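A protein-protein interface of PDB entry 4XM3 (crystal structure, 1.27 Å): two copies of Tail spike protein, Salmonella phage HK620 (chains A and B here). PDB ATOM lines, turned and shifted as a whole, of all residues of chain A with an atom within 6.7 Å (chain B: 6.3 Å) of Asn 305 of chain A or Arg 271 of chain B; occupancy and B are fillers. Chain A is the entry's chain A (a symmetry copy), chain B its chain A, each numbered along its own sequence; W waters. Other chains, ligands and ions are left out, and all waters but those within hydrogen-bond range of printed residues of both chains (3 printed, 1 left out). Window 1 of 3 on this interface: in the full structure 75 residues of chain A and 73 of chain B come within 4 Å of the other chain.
NH1 of Arg 271 of chain B sits at hydrogen-bond distance from O of Gly 272 of chain A, 3.0 Å away.
The side-chain amide nitrogen (ND2) of Asn 305 of chain A lies close to the side-chain amide nitrogen (ND2) of Asn 305 of chain B.
The side-chain carboxylate (OE1) of Glu 304 of chain B lies close to the side-chain amide oxygen (OD1) of Asn 305 of chain A (2.7 Å).
OE2 of Glu 304 of chain B sits close to O of Gly 336 of chain A (2.7 Å).
The side-chain amide nitrogen (NE2) of Gln 302 of chain B sits at hydrogen-bond distance from the backbone carbonyl oxygen (O) of Asn 305 of chain A, 3.0 Å away.
The side-chain hydroxyl (OG) of Ser 244 of chain A is in hydrogen-bond range of the side-chain carboxylate (OE1) of Glu 243 of chain B, at 3.0 Å.
O of Ser 273 of chain A lies within hydrogen-bond range of N of Ile 307 of chain A.
O of Tyr 270 of chain B is in hydrogen-bond range of N of Glu 304 of chain B (3.0 Å).
O of Ser 335 of chain A lies within hydrogen-bond range of N of Asn 305 of chain A (3.0 Å).
N of Tyr 270 of chain B is in hydrogen-bond range of O of Gln 302 of chain B, at 2.9 Å.
The backbone NH of Ser 244 of chain A is in hydrogen-bond range of the backbone carbonyl oxygen of Arg 271 of chain A.
The backbone NH (N) of Asn 305 of chain A is in hydrogen-bond range of the side-chain amide oxygen (OD1) of Asn 337 of chain A, at 3.4 Å.
Arg 271 of chain B touches Asn 305 of chain A.
Ile 307 of chain A touches Arg 271 of chain B (CD1 to NH2, 3.8 Å).
OE1 of Gln 302 of chain B touches CD1 of Ile 307 of chain A (3.7 Å).
Of the printed residues of chain B, Asn 305 of chain A touches Arg 271, Gln 302, Glu 304 and Asn 305.
Of the printed residues of chain A, Arg 271 of chain B touches Gly 272, Asn 305 and Ile 307.
Of the printed residues of chain A, Glu 243 of chain B touches Ser 244.
Of the printed residues of chain A, Asn 305 of chain B touches Asn 305 (3.4 Å).
Of the printed residues of chain B, Ser 244 of chain A touches Glu 243.
Printed residues of chain A within 4 Å of Glu 304 of chain B: Asn 305 (2.7 Å) and Gly 336 (2.7 Å).
Printed residues of chain B within 4 Å of Ile 307 of chain A: Arg 271 (3.8 Å) and Gln 302 (3.7 Å).
Ser 273 of chain B touches none of the printed residues of chain A.
Ser 244 of chain B touches none of the printed residues of chain A.
The nearest printed residue of chain B that does not touch Asn 305 of chain A is Ser 335 of chain B (5.6 Å).
The nearest printed residue of chain A that does not touch Arg 271 of chain B is Ser 273 of chain A (4.2 Å).
The nearest printed residue of chain B that does not touch Ile 307 of chain A is Phe 269 of chain B (4.2 Å).
Along chain B the printed residues that touch a printed residue of chain A span positions 243 to 305.
Printed residues of chain A that touch a printed residue of chain B: Ser 244, Gly 272, Asn 305, Ile 307 and Gly 336.
Hydrophobic or aromatic side chains of chain A that line the printed part of chain B: Ile 307.
Among the printed residues, 9 pairs touch across the chains.
Among the printed residues, no Asp or Glu carboxylate lies within 4 Å of a Lys or Arg side-chain nitrogen of the other chain.
Gly 272 of chain A touches Arg 271 of chain B, but with the chains exchanged Arg 271 of chain A does not touch Gly 272 of chain B (11.0 Å).
Asn 305 of chain A touches Arg 271 of chain B, but with the chains exchanged Arg 271 of chain A does not touch Asn 305 of chain B (8.2 Å).
Asn 305 of chain A touches Glu 304 of chain B, but with the chains exchanged Glu 304 of chain A does not touch Asn 305 of chain B (7.0 Å).
Asn 305 of chain B touches its own counterpart, Asn 305 of chain A.
Positions printed for both chains: 244, 270, 271, 272, 273, 303, 304, 305, 306 and 335.
Of the 9 pairs that touch across the chains among the printed residues, 1 has its exchanged pair printed and touching as well.
Water W2 lies within hydrogen-bond range of the guanidinium group of Arg 271 of chain B, the side-chain hydroxyl of Thr 274 of chain A and the backbone carbonyl oxygen of Gly 272 of chain A.
Water W1 lies within hydrogen-bond range of OG of Ser 335 of chain B (2.8 Å), O of Gly 377 of chain A (2.9 Å), OG of Ser 335 of chain A (3.4 Å) and N of Gly 336 of chain A (3.4 Å).
Water W3 lies within hydrogen-bond range of the side-chain amide oxygen of Asn 305 of chain A (2.9 Å), the side-chain amide nitrogen of Asn 305 of chain B (3.3 Å) and the side-chain hydroxyl of Ser 335 of chain B (3.4 Å).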
ATOM      1  N   SER A 244      15.839 -15.847  20.798  1.00  0.00           N
ATOM      2  CA  SER A 244      15.305 -15.143  21.986  1.00  0.00           C
ATOM      3  C   SER A 244      14.132 -14.256  21.580  1.00  0.00           C
ATOM      4  O   SER A 244      14.068 -13.115  22.056  1.00  0.00           O
ATOM      5  CB  SER A 244      16.390 -14.387  22.759  1.00  0.00           C
ATOM      6  OG  SER A 244      17.364 -15.294  23.231  1.00  0.00           O
ATOM      7  N   TYR A 270      17.236 -21.420  14.871  1.00  0.00           N
ATOM      8  CA  TYR A 270      16.067 -20.955  15.622  1.00  0.00           C
ATOM      9  C   TYR A 270      16.240 -21.422  17.058  1.00  0.00           C
ATOM     10  O   TYR A 270      16.155 -22.642  17.334  1.00  0.00           O
ATOM     11  CB  TYR A 270      14.791 -21.438  14.992  1.00  0.00           C
ATOM     12  CG  TYR A 270      13.548 -21.062  15.658  1.00  0.00           C
ATOM     13  CD1 TYR A 270      13.416 -19.857  16.373  1.00  0.00           C
ATOM     14  CD2 TYR A 270      12.420 -21.810  15.506  1.00  0.00           C
ATOM     15  CE1 TYR A 270      12.216 -19.469  16.926  1.00  0.00           C
ATOM     16  CE2 TYR A 270      11.245 -21.439  16.093  1.00  0.00           C
ATOM     17  CZ  TYR A 270      11.124 -20.220  16.788  1.00  0.00           C
ATOM     18  OH  TYR A 270       9.912 -19.822  17.301  1.00  0.00           O
ATOM     19  N   ARG A 271      16.476 -20.477  17.967  1.00  0.00           N
ATOM     20  CA  ARG A 271      16.914 -20.805  19.323  1.00  0.00           C
ATOM     21  C   ARG A 271      16.204 -19.982  20.376  1.00  0.00           C
ATOM     22  O   ARG A 271      15.891 -18.788  20.162  1.00  0.00           O
ATOM     23  CB  ARG A 271      18.449 -20.511  19.485  1.00  0.00           C
ATOM     24  CG  ARG A 271      19.455 -21.404  18.694  1.00  0.00           C
ATOM     25  CD  ARG A 271      20.917 -21.260  19.220  1.00  0.00           C
ATOM     26  NE  ARG A 271      21.990 -21.550  18.225  1.00  0.00           N
ATOM     27  CZ  ARG A 271      22.776 -20.654  17.596  1.00  0.00           C
ATOM     28  NH1 ARG A 271      22.686 -19.321  17.803  1.00  0.00           N
ATOM     29  NH2 ARG A 271      23.715 -21.110  16.755  1.00  0.00           N
ATOM     30  N   GLY A 272      16.007 -20.568  21.557  1.00  0.00           N
ATOM     31  CA  GLY A 272      15.680 -19.784  22.760  1.00  0.00           C
ATOM     32  C   GLY A 272      14.399 -18.983  22.657  1.00  0.00           C
ATOM     33  O   GLY A 272      14.298 -17.955  23.341  1.00  0.00           O
ATOM     34  N   SER A 273      13.418 -19.405  21.840  1.00  0.00           N
ATOM     35  CA  SER A 273      12.231 -18.592  21.631  1.00  0.00           C
ATOM     36  C   SER A 273      11.006 -19.281  22.233  1.00  0.00           C
ATOM     37  O   SER A 273      11.033 -20.477  22.551  1.00  0.00           O
ATOM     38  CB  SER A 273      12.066 -18.329  20.133  1.00  0.00           C
ATOM     39  OG  SER A 273      13.191 -17.586  19.649  1.00  0.00           O
ATOM     40  N   THR A 274       9.937 -18.491  22.447  1.00  0.00           N
ATOM     41  CA  THR A 274       8.679 -18.962  22.998  1.00  0.00           C
ATOM     42  C   THR A 274       7.585 -18.694  21.987  1.00  0.00           C
ATOM     43  O   THR A 274       7.478 -17.580  21.480  1.00  0.00           O
ATOM     44  CB  THR A 274       8.410 -18.280  24.365  1.00  0.00           C
ATOM     45  OG1 THR A 274       9.395 -18.637  25.319  1.00  0.00           O
ATOM     46  CG2 THR A 274       7.054 -18.733  24.870  1.00  0.00           C
ATOM     47  N   VAL A 303      17.497 -26.226  15.510  1.00  0.00           N
ATOM     48  CA  VAL A 303      16.306 -25.797  16.231  1.00  0.00           C
ATOM     49  C   VAL A 303      16.499 -26.237  17.688  1.00  0.00           C
ATOM     50  O   VAL A 303      16.344 -27.436  17.986  1.00  0.00           O
ATOM     51  CB  VAL A 303      15.041 -26.408  15.621  1.00  0.00           C
ATOM     52  CG1 VAL A 303      13.825 -25.917  16.403  1.00  0.00           C
ATOM     53  CG2 VAL A 303      14.848 -26.044  14.206  1.00  0.00           C
ATOM     54  N   GLU A 304      16.771 -25.286  18.604  1.00  0.00           N
ATOM     55  CA  GLU A 304      17.236 -25.628  19.942  1.00  0.00           C
ATOM     56  C   GLU A 304      16.654 -24.754  21.029  1.00  0.00           C
ATOM     57  O   GLU A 304      16.526 -23.521  20.904  1.00  0.00           O
ATOM     58  CB  GLU A 304      18.779 -25.585  20.094  1.00  0.00           C
ATOM     59  CG  GLU A 304      19.432 -26.737  19.397  1.00  0.00           C
ATOM     60  CD  GLU A 304      20.957 -26.856  19.506  1.00  0.00           C
ATOM     61  OE1 GLU A 304      21.632 -25.841  19.702  1.00  0.00           O
ATOM     62  OE2 GLU A 304      21.465 -27.967  19.320  1.00  0.00           O
ATOM     63  N   ASN A 305      16.280 -25.398  22.119  1.00  0.00           N
ATOM     64  CA  ASN A 305      15.993 -24.676  23.387  1.00  0.00           C
ATOM     65  C   ASN A 305      14.808 -23.724  23.251  1.00  0.00           C
ATOM     66  O   ASN A 305      14.776 -22.694  23.919  1.00  0.00           O
ATOM     67  CB  ASN A 305      17.235 -24.017  23.949  1.00  0.00           C
ATOM     68  CG  ASN A 305      18.322 -25.095  24.265  1.00  0.00           C
ATOM     69  OD1 ASN A 305      18.070 -26.134  24.767  1.00  0.00           O
ATOM     70  ND2 ASN A 305      19.440 -24.896  23.756  1.00  0.00           N
ATOM     71  N   ASN A 306      13.809 -24.103  22.453  1.00  0.00           N
ATOM     72  CA  ASN A 306      12.540 -23.355  22.337  1.00  0.00           C
ATOM     73  C   ASN A 306      11.446 -23.925  23.231  1.00  0.00           C
ATOM     74  O   ASN A 306      11.526 -25.068  23.661  1.00  0.00           O
ATOM     75  CB  ASN A 306      12.084 -23.304  20.889  1.00  0.00           C
ATOM     76  CG  ASN A 306      13.180 -22.720  19.987  1.00  0.00           C
ATOM     77  OD1 ASN A 306      13.469 -21.517  20.025  1.00  0.00           O
ATOM     78  ND2 ASN A 306      13.713 -23.540  19.064  1.00  0.00           N
ATOM     79  N   ILE A 307      10.469 -23.074  23.478  1.00  0.00           N
ATOM     80  CA  ILE A 307       9.327 -23.412  24.277  1.00  0.00           C
ATOM     81  C   ILE A 307       8.091 -23.189  23.382  1.00  0.00           C
ATOM     82  O   ILE A 307       7.972 -22.104  22.818  1.00  0.00           O
ATOM     83  CB  ILE A 307       9.239 -22.504  25.504  1.00  0.00           C
ATOM     84  CG1 ILE A 307      10.494 -22.609  26.377  1.00  0.00           C
ATOM     85  CG2 ILE A 307       7.967 -22.791  26.237  1.00  0.00           C
ATOM     86  CD1 ILE A 307      10.505 -21.581  27.509  1.00  0.00           C
ATOM     87  N   VAL A 334      17.748 -30.998  16.319  1.00  0.00           N
ATOM     88  CA  VAL A 334      16.570 -30.547  17.071  1.00  0.00           C
ATOM     89  C   VAL A 334      16.742 -30.984  18.487  1.00  0.00           C
ATOM     90  O   VAL A 334      16.660 -32.202  18.729  1.00  0.00           O
ATOM     91  CB  VAL A 334      15.302 -31.074  16.438  1.00  0.00           C
ATOM     92  CG1 VAL A 334      14.081 -30.604  17.239  1.00  0.00           C
ATOM     93  CG2 VAL A 334      15.179 -30.737  14.915  1.00  0.00           C
ATOM     94  N   SER A 335      17.104 -30.060  19.389  1.00  0.00           N
ATOM     95  CA  SER A 335      17.455 -30.460  20.763  1.00  0.00           C
ATOM     96  C   SER A 335      16.983 -29.444  21.776  1.00  0.00           C
ATOM     97  O   SER A 335      16.947 -28.237  21.516  1.00  0.00           O
ATOM     98  CB  SER A 335      18.994 -30.598  20.912  1.00  0.00           C
ATOM     99  OG  SER A 335      19.324 -31.145  22.190  1.00  0.00           O
ATOM    100  N   GLY A 336      16.653 -29.945  22.959  1.00  0.00           N
ATOM    101  CA  GLY A 336      16.367 -29.072  24.113  1.00  0.00           C
ATOM    102  C   GLY A 336      15.017 -28.372  24.087  1.00  0.00           C
ATOM    103  O   GLY A 336      14.793 -27.461  24.898  1.00  0.00           O
ATOM    104  N   ASN A 337      14.145 -28.722  23.124  1.00  0.00           N
ATOM    105  CA  ASN A 337      12.856 -28.046  23.027  1.00  0.00           C
ATOM    106  C   ASN A 337      11.820 -28.691  23.961  1.00  0.00           C
ATOM    107  O   ASN A 337      11.857 -29.893  24.162  1.00  0.00           O
ATOM    108  CB  ASN A 337      12.336 -28.093  21.576  1.00  0.00           C
ATOM    109  CG  ASN A 337      13.344 -27.469  20.597  1.00  0.00           C
ATOM    110  OD1 ASN A 337      13.472 -26.269  20.475  1.00  0.00           O
ATOM    111  ND2 ASN A 337      14.104 -28.329  19.888  1.00  0.00           N
ATOM    112  N   ILE A 338      10.942 -27.862  24.504  1.00  0.00           N
ATOM    113  CA  ILE A 338       9.841 -28.308  25.267  1.00  0.00           C
ATOM    114  C   ILE A 338       8.541 -27.859  24.590  1.00  0.00           C
ATOM    115  O   ILE A 338       8.336 -26.664  24.391  1.00  0.00           O
ATOM    116  CB  ILE A 338       9.887 -27.949  26.772  1.00  0.00           C
ATOM    117  CG1 ILE A 338       8.680 -28.469  27.499  1.00  0.00           C
ATOM    118  CG2 ILE A 338      10.093 -26.471  27.032  1.00  0.00           C
ATOM    119  CD1 ILE A 338       8.826 -28.537  29.036  1.00  0.00           C
ATOM    120  N   GLY A 377      16.981 -35.049  23.287  1.00  0.00           N
ATOM    121  CA  GLY A 377      16.806 -34.246  24.500  1.00  0.00           C
ATOM    122  C   GLY A 377      15.683 -33.251  24.437  1.00  0.00           C
ATOM    123  O   GLY A 377      15.812 -32.152  24.982  1.00  0.00           O
ATOM    124  N   ASN A 378      14.584 -33.599  23.774  1.00  0.00           N
ATOM    125  CA  ASN A 378      13.357 -32.789  23.754  1.00  0.00           C
ATOM    126  C   ASN A 378      12.251 -33.494  24.540  1.00  0.00           C
ATOM    127  O   ASN A 378      12.286 -34.706  24.769  1.00  0.00           O
ATOM    128  CB  ASN A 378      12.835 -32.695  22.278  1.00  0.00           C
ATOM    129  CG  ASN A 378      13.869 -32.176  21.295  1.00  0.00           C
ATOM    130  OD1 ASN A 378      14.092 -30.967  21.237  1.00  0.00           O
ATOM    131  ND2 ASN A 378      14.508 -33.064  20.562  1.00  0.00           N
ATOM    132  N   VAL B 242      15.085 -15.223  32.549  1.00  0.00           N
ATOM    133  CA  VAL B 242      16.424 -14.784  32.839  1.00  0.00           C
ATOM    134  C   VAL B 242      17.413 -15.437  31.896  1.00  0.00           C
ATOM    135  O   VAL B 242      17.407 -16.669  31.755  1.00  0.00           O
ATOM    136  CB  VAL B 242      16.761 -15.149  34.278  1.00  0.00           C
ATOM    137  CG1 VAL B 242      18.188 -14.705  34.616  1.00  0.00           C
ATOM    138  CG2 VAL B 242      15.804 -14.475  35.222  1.00  0.00           C
ATOM    139  N   GLU B 243      18.270 -14.640  31.243  1.00  0.00           N
ATOM    140  CA  GLU B 243      19.253 -15.223  30.354  1.00  0.00           C
ATOM    141  C   GLU B 243      20.586 -14.509  30.387  1.00  0.00           C
ATOM    142  O   GLU B 243      20.614 -13.265  30.508  1.00  0.00           O
ATOM    143  CB  GLU B 243      18.691 -15.440  28.960  1.00  0.00           C
ATOM    144  CG  GLU B 243      18.391 -14.276  28.103  1.00  0.00           C
ATOM    145  CD  GLU B 243      17.591 -14.614  26.775  1.00  0.00           C
ATOM    146  OE1 GLU B 243      17.826 -15.664  26.157  1.00  0.00           O
ATOM    147  OE2 GLU B 243      16.712 -13.791  26.324  1.00  0.00           O
ATOM    148  N   SER B 244      21.651 -15.279  30.363  1.00  0.00           N
ATOM    149  CA  SER B 244      23.025 -14.757  30.179  1.00  0.00           C
ATOM    150  C   SER B 244      23.371 -13.799  31.316  1.00  0.00           C
ATOM    151  O   SER B 244      23.953 -12.743  31.035  1.00  0.00           O
ATOM    152  CB  SER B 244      23.242 -14.145  28.792  1.00  0.00           C
ATOM    153  OG  SER B 244      23.049 -15.128  27.798  1.00  0.00           O
ATOM    154  N   CYS B 245      23.094 -14.186  32.545  1.00  0.00           N
ATOM    155  CA  CYS B 245      23.422 -13.383  33.726  1.00  0.00           C
ATOM    156  C   CYS B 245      24.536 -14.029  34.546  1.00  0.00           C
ATOM    157  O   CYS B 245      24.873 -15.216  34.328  1.00  0.00           O
ATOM    158  CB  CYS B 245      22.177 -13.166  34.612  1.00  0.00           C
ATOM    159  SG  CYS B 245      20.957 -12.062  33.878  1.00  0.00           S
ATOM    160  N   PHE B 269      11.693 -19.169  31.890  1.00  0.00           N
ATOM    161  CA  PHE B 269      12.959 -19.742  31.621  1.00  0.00           C
ATOM    162  C   PHE B 269      14.133 -19.148  32.400  1.00  0.00           C
ATOM    163  O   PHE B 269      14.108 -17.954  32.762  1.00  0.00           O
ATOM    164  CB  PHE B 269      13.256 -19.723  30.144  1.00  0.00           C
ATOM    165  CG  PHE B 269      13.366 -18.321  29.529  1.00  0.00           C
ATOM    166  CD1 PHE B 269      14.515 -17.591  29.570  1.00  0.00           C
ATOM    167  CD2 PHE B 269      12.313 -17.789  28.862  1.00  0.00           C
ATOM    168  CE1 PHE B 269      14.584 -16.323  28.999  1.00  0.00           C
ATOM    169  CE2 PHE B 269      12.340 -16.492  28.333  1.00  0.00           C
ATOM    170  CZ  PHE B 269      13.528 -15.801  28.361  1.00  0.00           C
ATOM    171  N   TYR B 270      15.177 -19.906  32.556  1.00  0.00           N
ATOM    172  CA  TYR B 270      16.462 -19.542  33.160  1.00  0.00           C
ATOM    173  C   TYR B 270      17.550 -20.224  32.348  1.00  0.00           C
ATOM    174  O   TYR B 270      17.678 -21.471  32.396  1.00  0.00           O
ATOM    175  CB  TYR B 270      16.497 -19.902  34.618  1.00  0.00           C
ATOM    176  CG  TYR B 270      17.734 -19.612  35.336  1.00  0.00           C
ATOM    177  CD1 TYR B 270      18.563 -18.528  34.992  1.00  0.00           C
ATOM    178  CD2 TYR B 270      18.072 -20.310  36.456  1.00  0.00           C
ATOM    179  CE1 TYR B 270      19.684 -18.210  35.726  1.00  0.00           C
ATOM    180  CE2 TYR B 270      19.207 -20.014  37.154  1.00  0.00           C
ATOM    181  CZ  TYR B 270      20.016 -18.913  36.808  1.00  0.00           C
ATOM    182  OH  TYR B 270      21.108 -18.578  37.572  1.00  0.00           O
ATOM    183  N   ARG B 271      18.330 -19.433  31.614  1.00  0.00           N
ATOM    184  CA  ARG B 271      19.235 -19.971  30.598  1.00  0.00           C
ATOM    185  C   ARG B 271      20.595 -19.307  30.625  1.00  0.00           C
ATOM    186  O   ARG B 271      20.715 -18.089  30.893  1.00  0.00           O
ATOM    187  CB  ARG B 271      18.646 -19.730  29.162  1.00  0.00           C
ATOM    188  CG  ARG B 271      17.356 -20.509  28.758  1.00  0.00           C
ATOM    189  CD  ARG B 271      17.096 -20.470  27.220  1.00  0.00           C
ATOM    190  NE  ARG B 271      15.672 -20.623  26.803  1.00  0.00           N
ATOM    191  CZ  ARG B 271      14.852 -19.654  26.349  1.00  0.00           C
ATOM    192  NH1 ARG B 271      15.240 -18.367  26.205  1.00  0.00           N
ATOM    193  NH2 ARG B 271      13.606 -19.992  25.988  1.00  0.00           N
ATOM    194  N   GLY B 272      21.633 -20.063  30.269  1.00  0.00           N
ATOM    195  CA  GLY B 272      22.927 -19.466  29.892  1.00  0.00           C
ATOM    196  C   GLY B 272      23.575 -18.639  30.982  1.00  0.00           C
ATOM    197  O   GLY B 272      24.341 -17.725  30.641  1.00  0.00           O
ATOM    198  N   SER B 273      23.310 -18.915  32.271  1.00  0.00           N
ATOM    199  CA  SER B 273      23.823 -18.060  33.328  1.00  0.00           C
ATOM    200  C   SER B 273      24.865 -18.814  34.158  1.00  0.00           C
ATOM    201  O   SER B 273      24.974 -20.044  34.085  1.00  0.00           O
ATOM    202  CB  SER B 273      22.652 -17.570  34.183  1.00  0.00           C
ATOM    203  OG  SER B 273      21.769 -16.780  33.377  1.00  0.00           O
ATOM    204  N   GLN B 302      11.675 -23.943  31.848  1.00  0.00           N
ATOM    205  CA  GLN B 302      12.952 -24.308  31.214  1.00  0.00           C
ATOM    206  C   GLN B 302      14.139 -23.834  32.033  1.00  0.00           C
ATOM    207  O   GLN B 302      14.270 -22.621  32.279  1.00  0.00           O
ATOM    208  CB  GLN B 302      13.025 -23.721  29.809  1.00  0.00           C
ATOM    209  CG  GLN B 302      14.205 -24.059  28.991  1.00  0.00           C
ATOM    210  CD  GLN B 302      14.139 -23.206  27.762  1.00  0.00           C
ATOM    211  OE1 GLN B 302      14.177 -22.028  27.847  1.00  0.00           O
ATOM    212  NE2 GLN B 302      14.054 -23.807  26.633  1.00  0.00           N
ATOM    213  N   VAL B 303      14.999 -24.757  32.449  1.00  0.00           N
ATOM    214  CA  VAL B 303      16.265 -24.423  33.090  1.00  0.00           C
ATOM    215  C   VAL B 303      17.364 -25.083  32.247  1.00  0.00           C
ATOM    216  O   VAL B 303      17.548 -26.311  32.344  1.00  0.00           O
ATOM    217  CB  VAL B 303      16.295 -24.914  34.540  1.00  0.00           C
ATOM    218  CG1 VAL B 303      17.633 -24.528  35.168  1.00  0.00           C
ATOM    219  CG2 VAL B 303      15.221 -24.335  35.368  1.00  0.00           C
ATOM    220  N   GLU B 304      18.132 -24.287  31.478  1.00  0.00           N
ATOM    221  CA  GLU B 304      19.006 -24.837  30.449  1.00  0.00           C
ATOM    222  C   GLU B 304      20.338 -24.129  30.342  1.00  0.00           C
ATOM    223  O   GLU B 304      20.447 -22.890  30.404  1.00  0.00           O
ATOM    224  CB  GLU B 304      18.374 -24.842  29.032  1.00  0.00           C
ATOM    225  CG  GLU B 304      17.307 -25.886  28.912  1.00  0.00           C
ATOM    226  CD  GLU B 304      16.626 -26.044  27.547  1.00  0.00           C
ATOM    227  OE1 GLU B 304      16.585 -25.082  26.775  1.00  0.00           O
ATOM    228  OE2 GLU B 304      16.077 -27.122  27.298  1.00  0.00           O
ATOM    229  N   ASN B 305      21.379 -24.926  30.190  1.00  0.00           N
ATOM    230  CA  ASN B 305      22.701 -24.402  29.753  1.00  0.00           C
ATOM    231  C   ASN B 305      23.292 -23.420  30.761  1.00  0.00           C
ATOM    232  O   ASN B 305      24.009 -22.504  30.369  1.00  0.00           O
ATOM    233  CB  ASN B 305      22.646 -23.856  28.341  1.00  0.00           C
ATOM    234  CG  ASN B 305      22.242 -24.987  27.341  1.00  0.00           C
ATOM    235  OD1 ASN B 305      22.669 -26.086  27.407  1.00  0.00           O
ATOM    236  ND2 ASN B 305      21.274 -24.731  26.603  1.00  0.00           N
ATOM    237  N   ASN B 306      23.058 -23.657  32.053  1.00  0.00           N
ATOM    238  CA  ASN B 306      23.683 -22.880  33.142  1.00  0.00           C
ATOM    239  C   ASN B 306      24.924 -23.561  33.704  1.00  0.00           C
ATOM    240  O   ASN B 306      25.112 -24.758  33.527  1.00  0.00           O
ATOM    241  CB  ASN B 306      22.674 -22.601  34.244  1.00  0.00           C
ATOM    242  CG  ASN B 306      21.426 -21.904  33.682  1.00  0.00           C
ATOM    243  OD1 ASN B 306      21.465 -20.726  33.305  1.00  0.00           O
ATOM    244  ND2 ASN B 306      20.268 -22.583  33.746  1.00  0.00           N
ATOM    245  N   SER B 335      18.047 -29.130  31.233  1.00  0.00           N
ATOM    246  CA  SER B 335      19.002 -29.740  30.291  1.00  0.00           C
ATOM    247  C   SER B 335      20.233 -28.883  30.113  1.00  0.00           C
ATOM    248  O   SER B 335      20.177 -27.650  30.163  1.00  0.00           O
ATOM    249  CB  SER B 335      18.347 -29.924  28.896  1.00  0.00           C
ATOM    250  OG  SER B 335      19.211 -30.666  28.033  1.00  0.00           O
HETATM  251  O   HOH W   1      18.524 -31.377  25.443  1.00  0.00           O
HETATM  252  O   HOH W   2      12.090 -17.860  25.122  1.00  0.00           O
HETATM  253  O   HOH W   3      19.776 -27.619  26.653  1.00  0.00           O
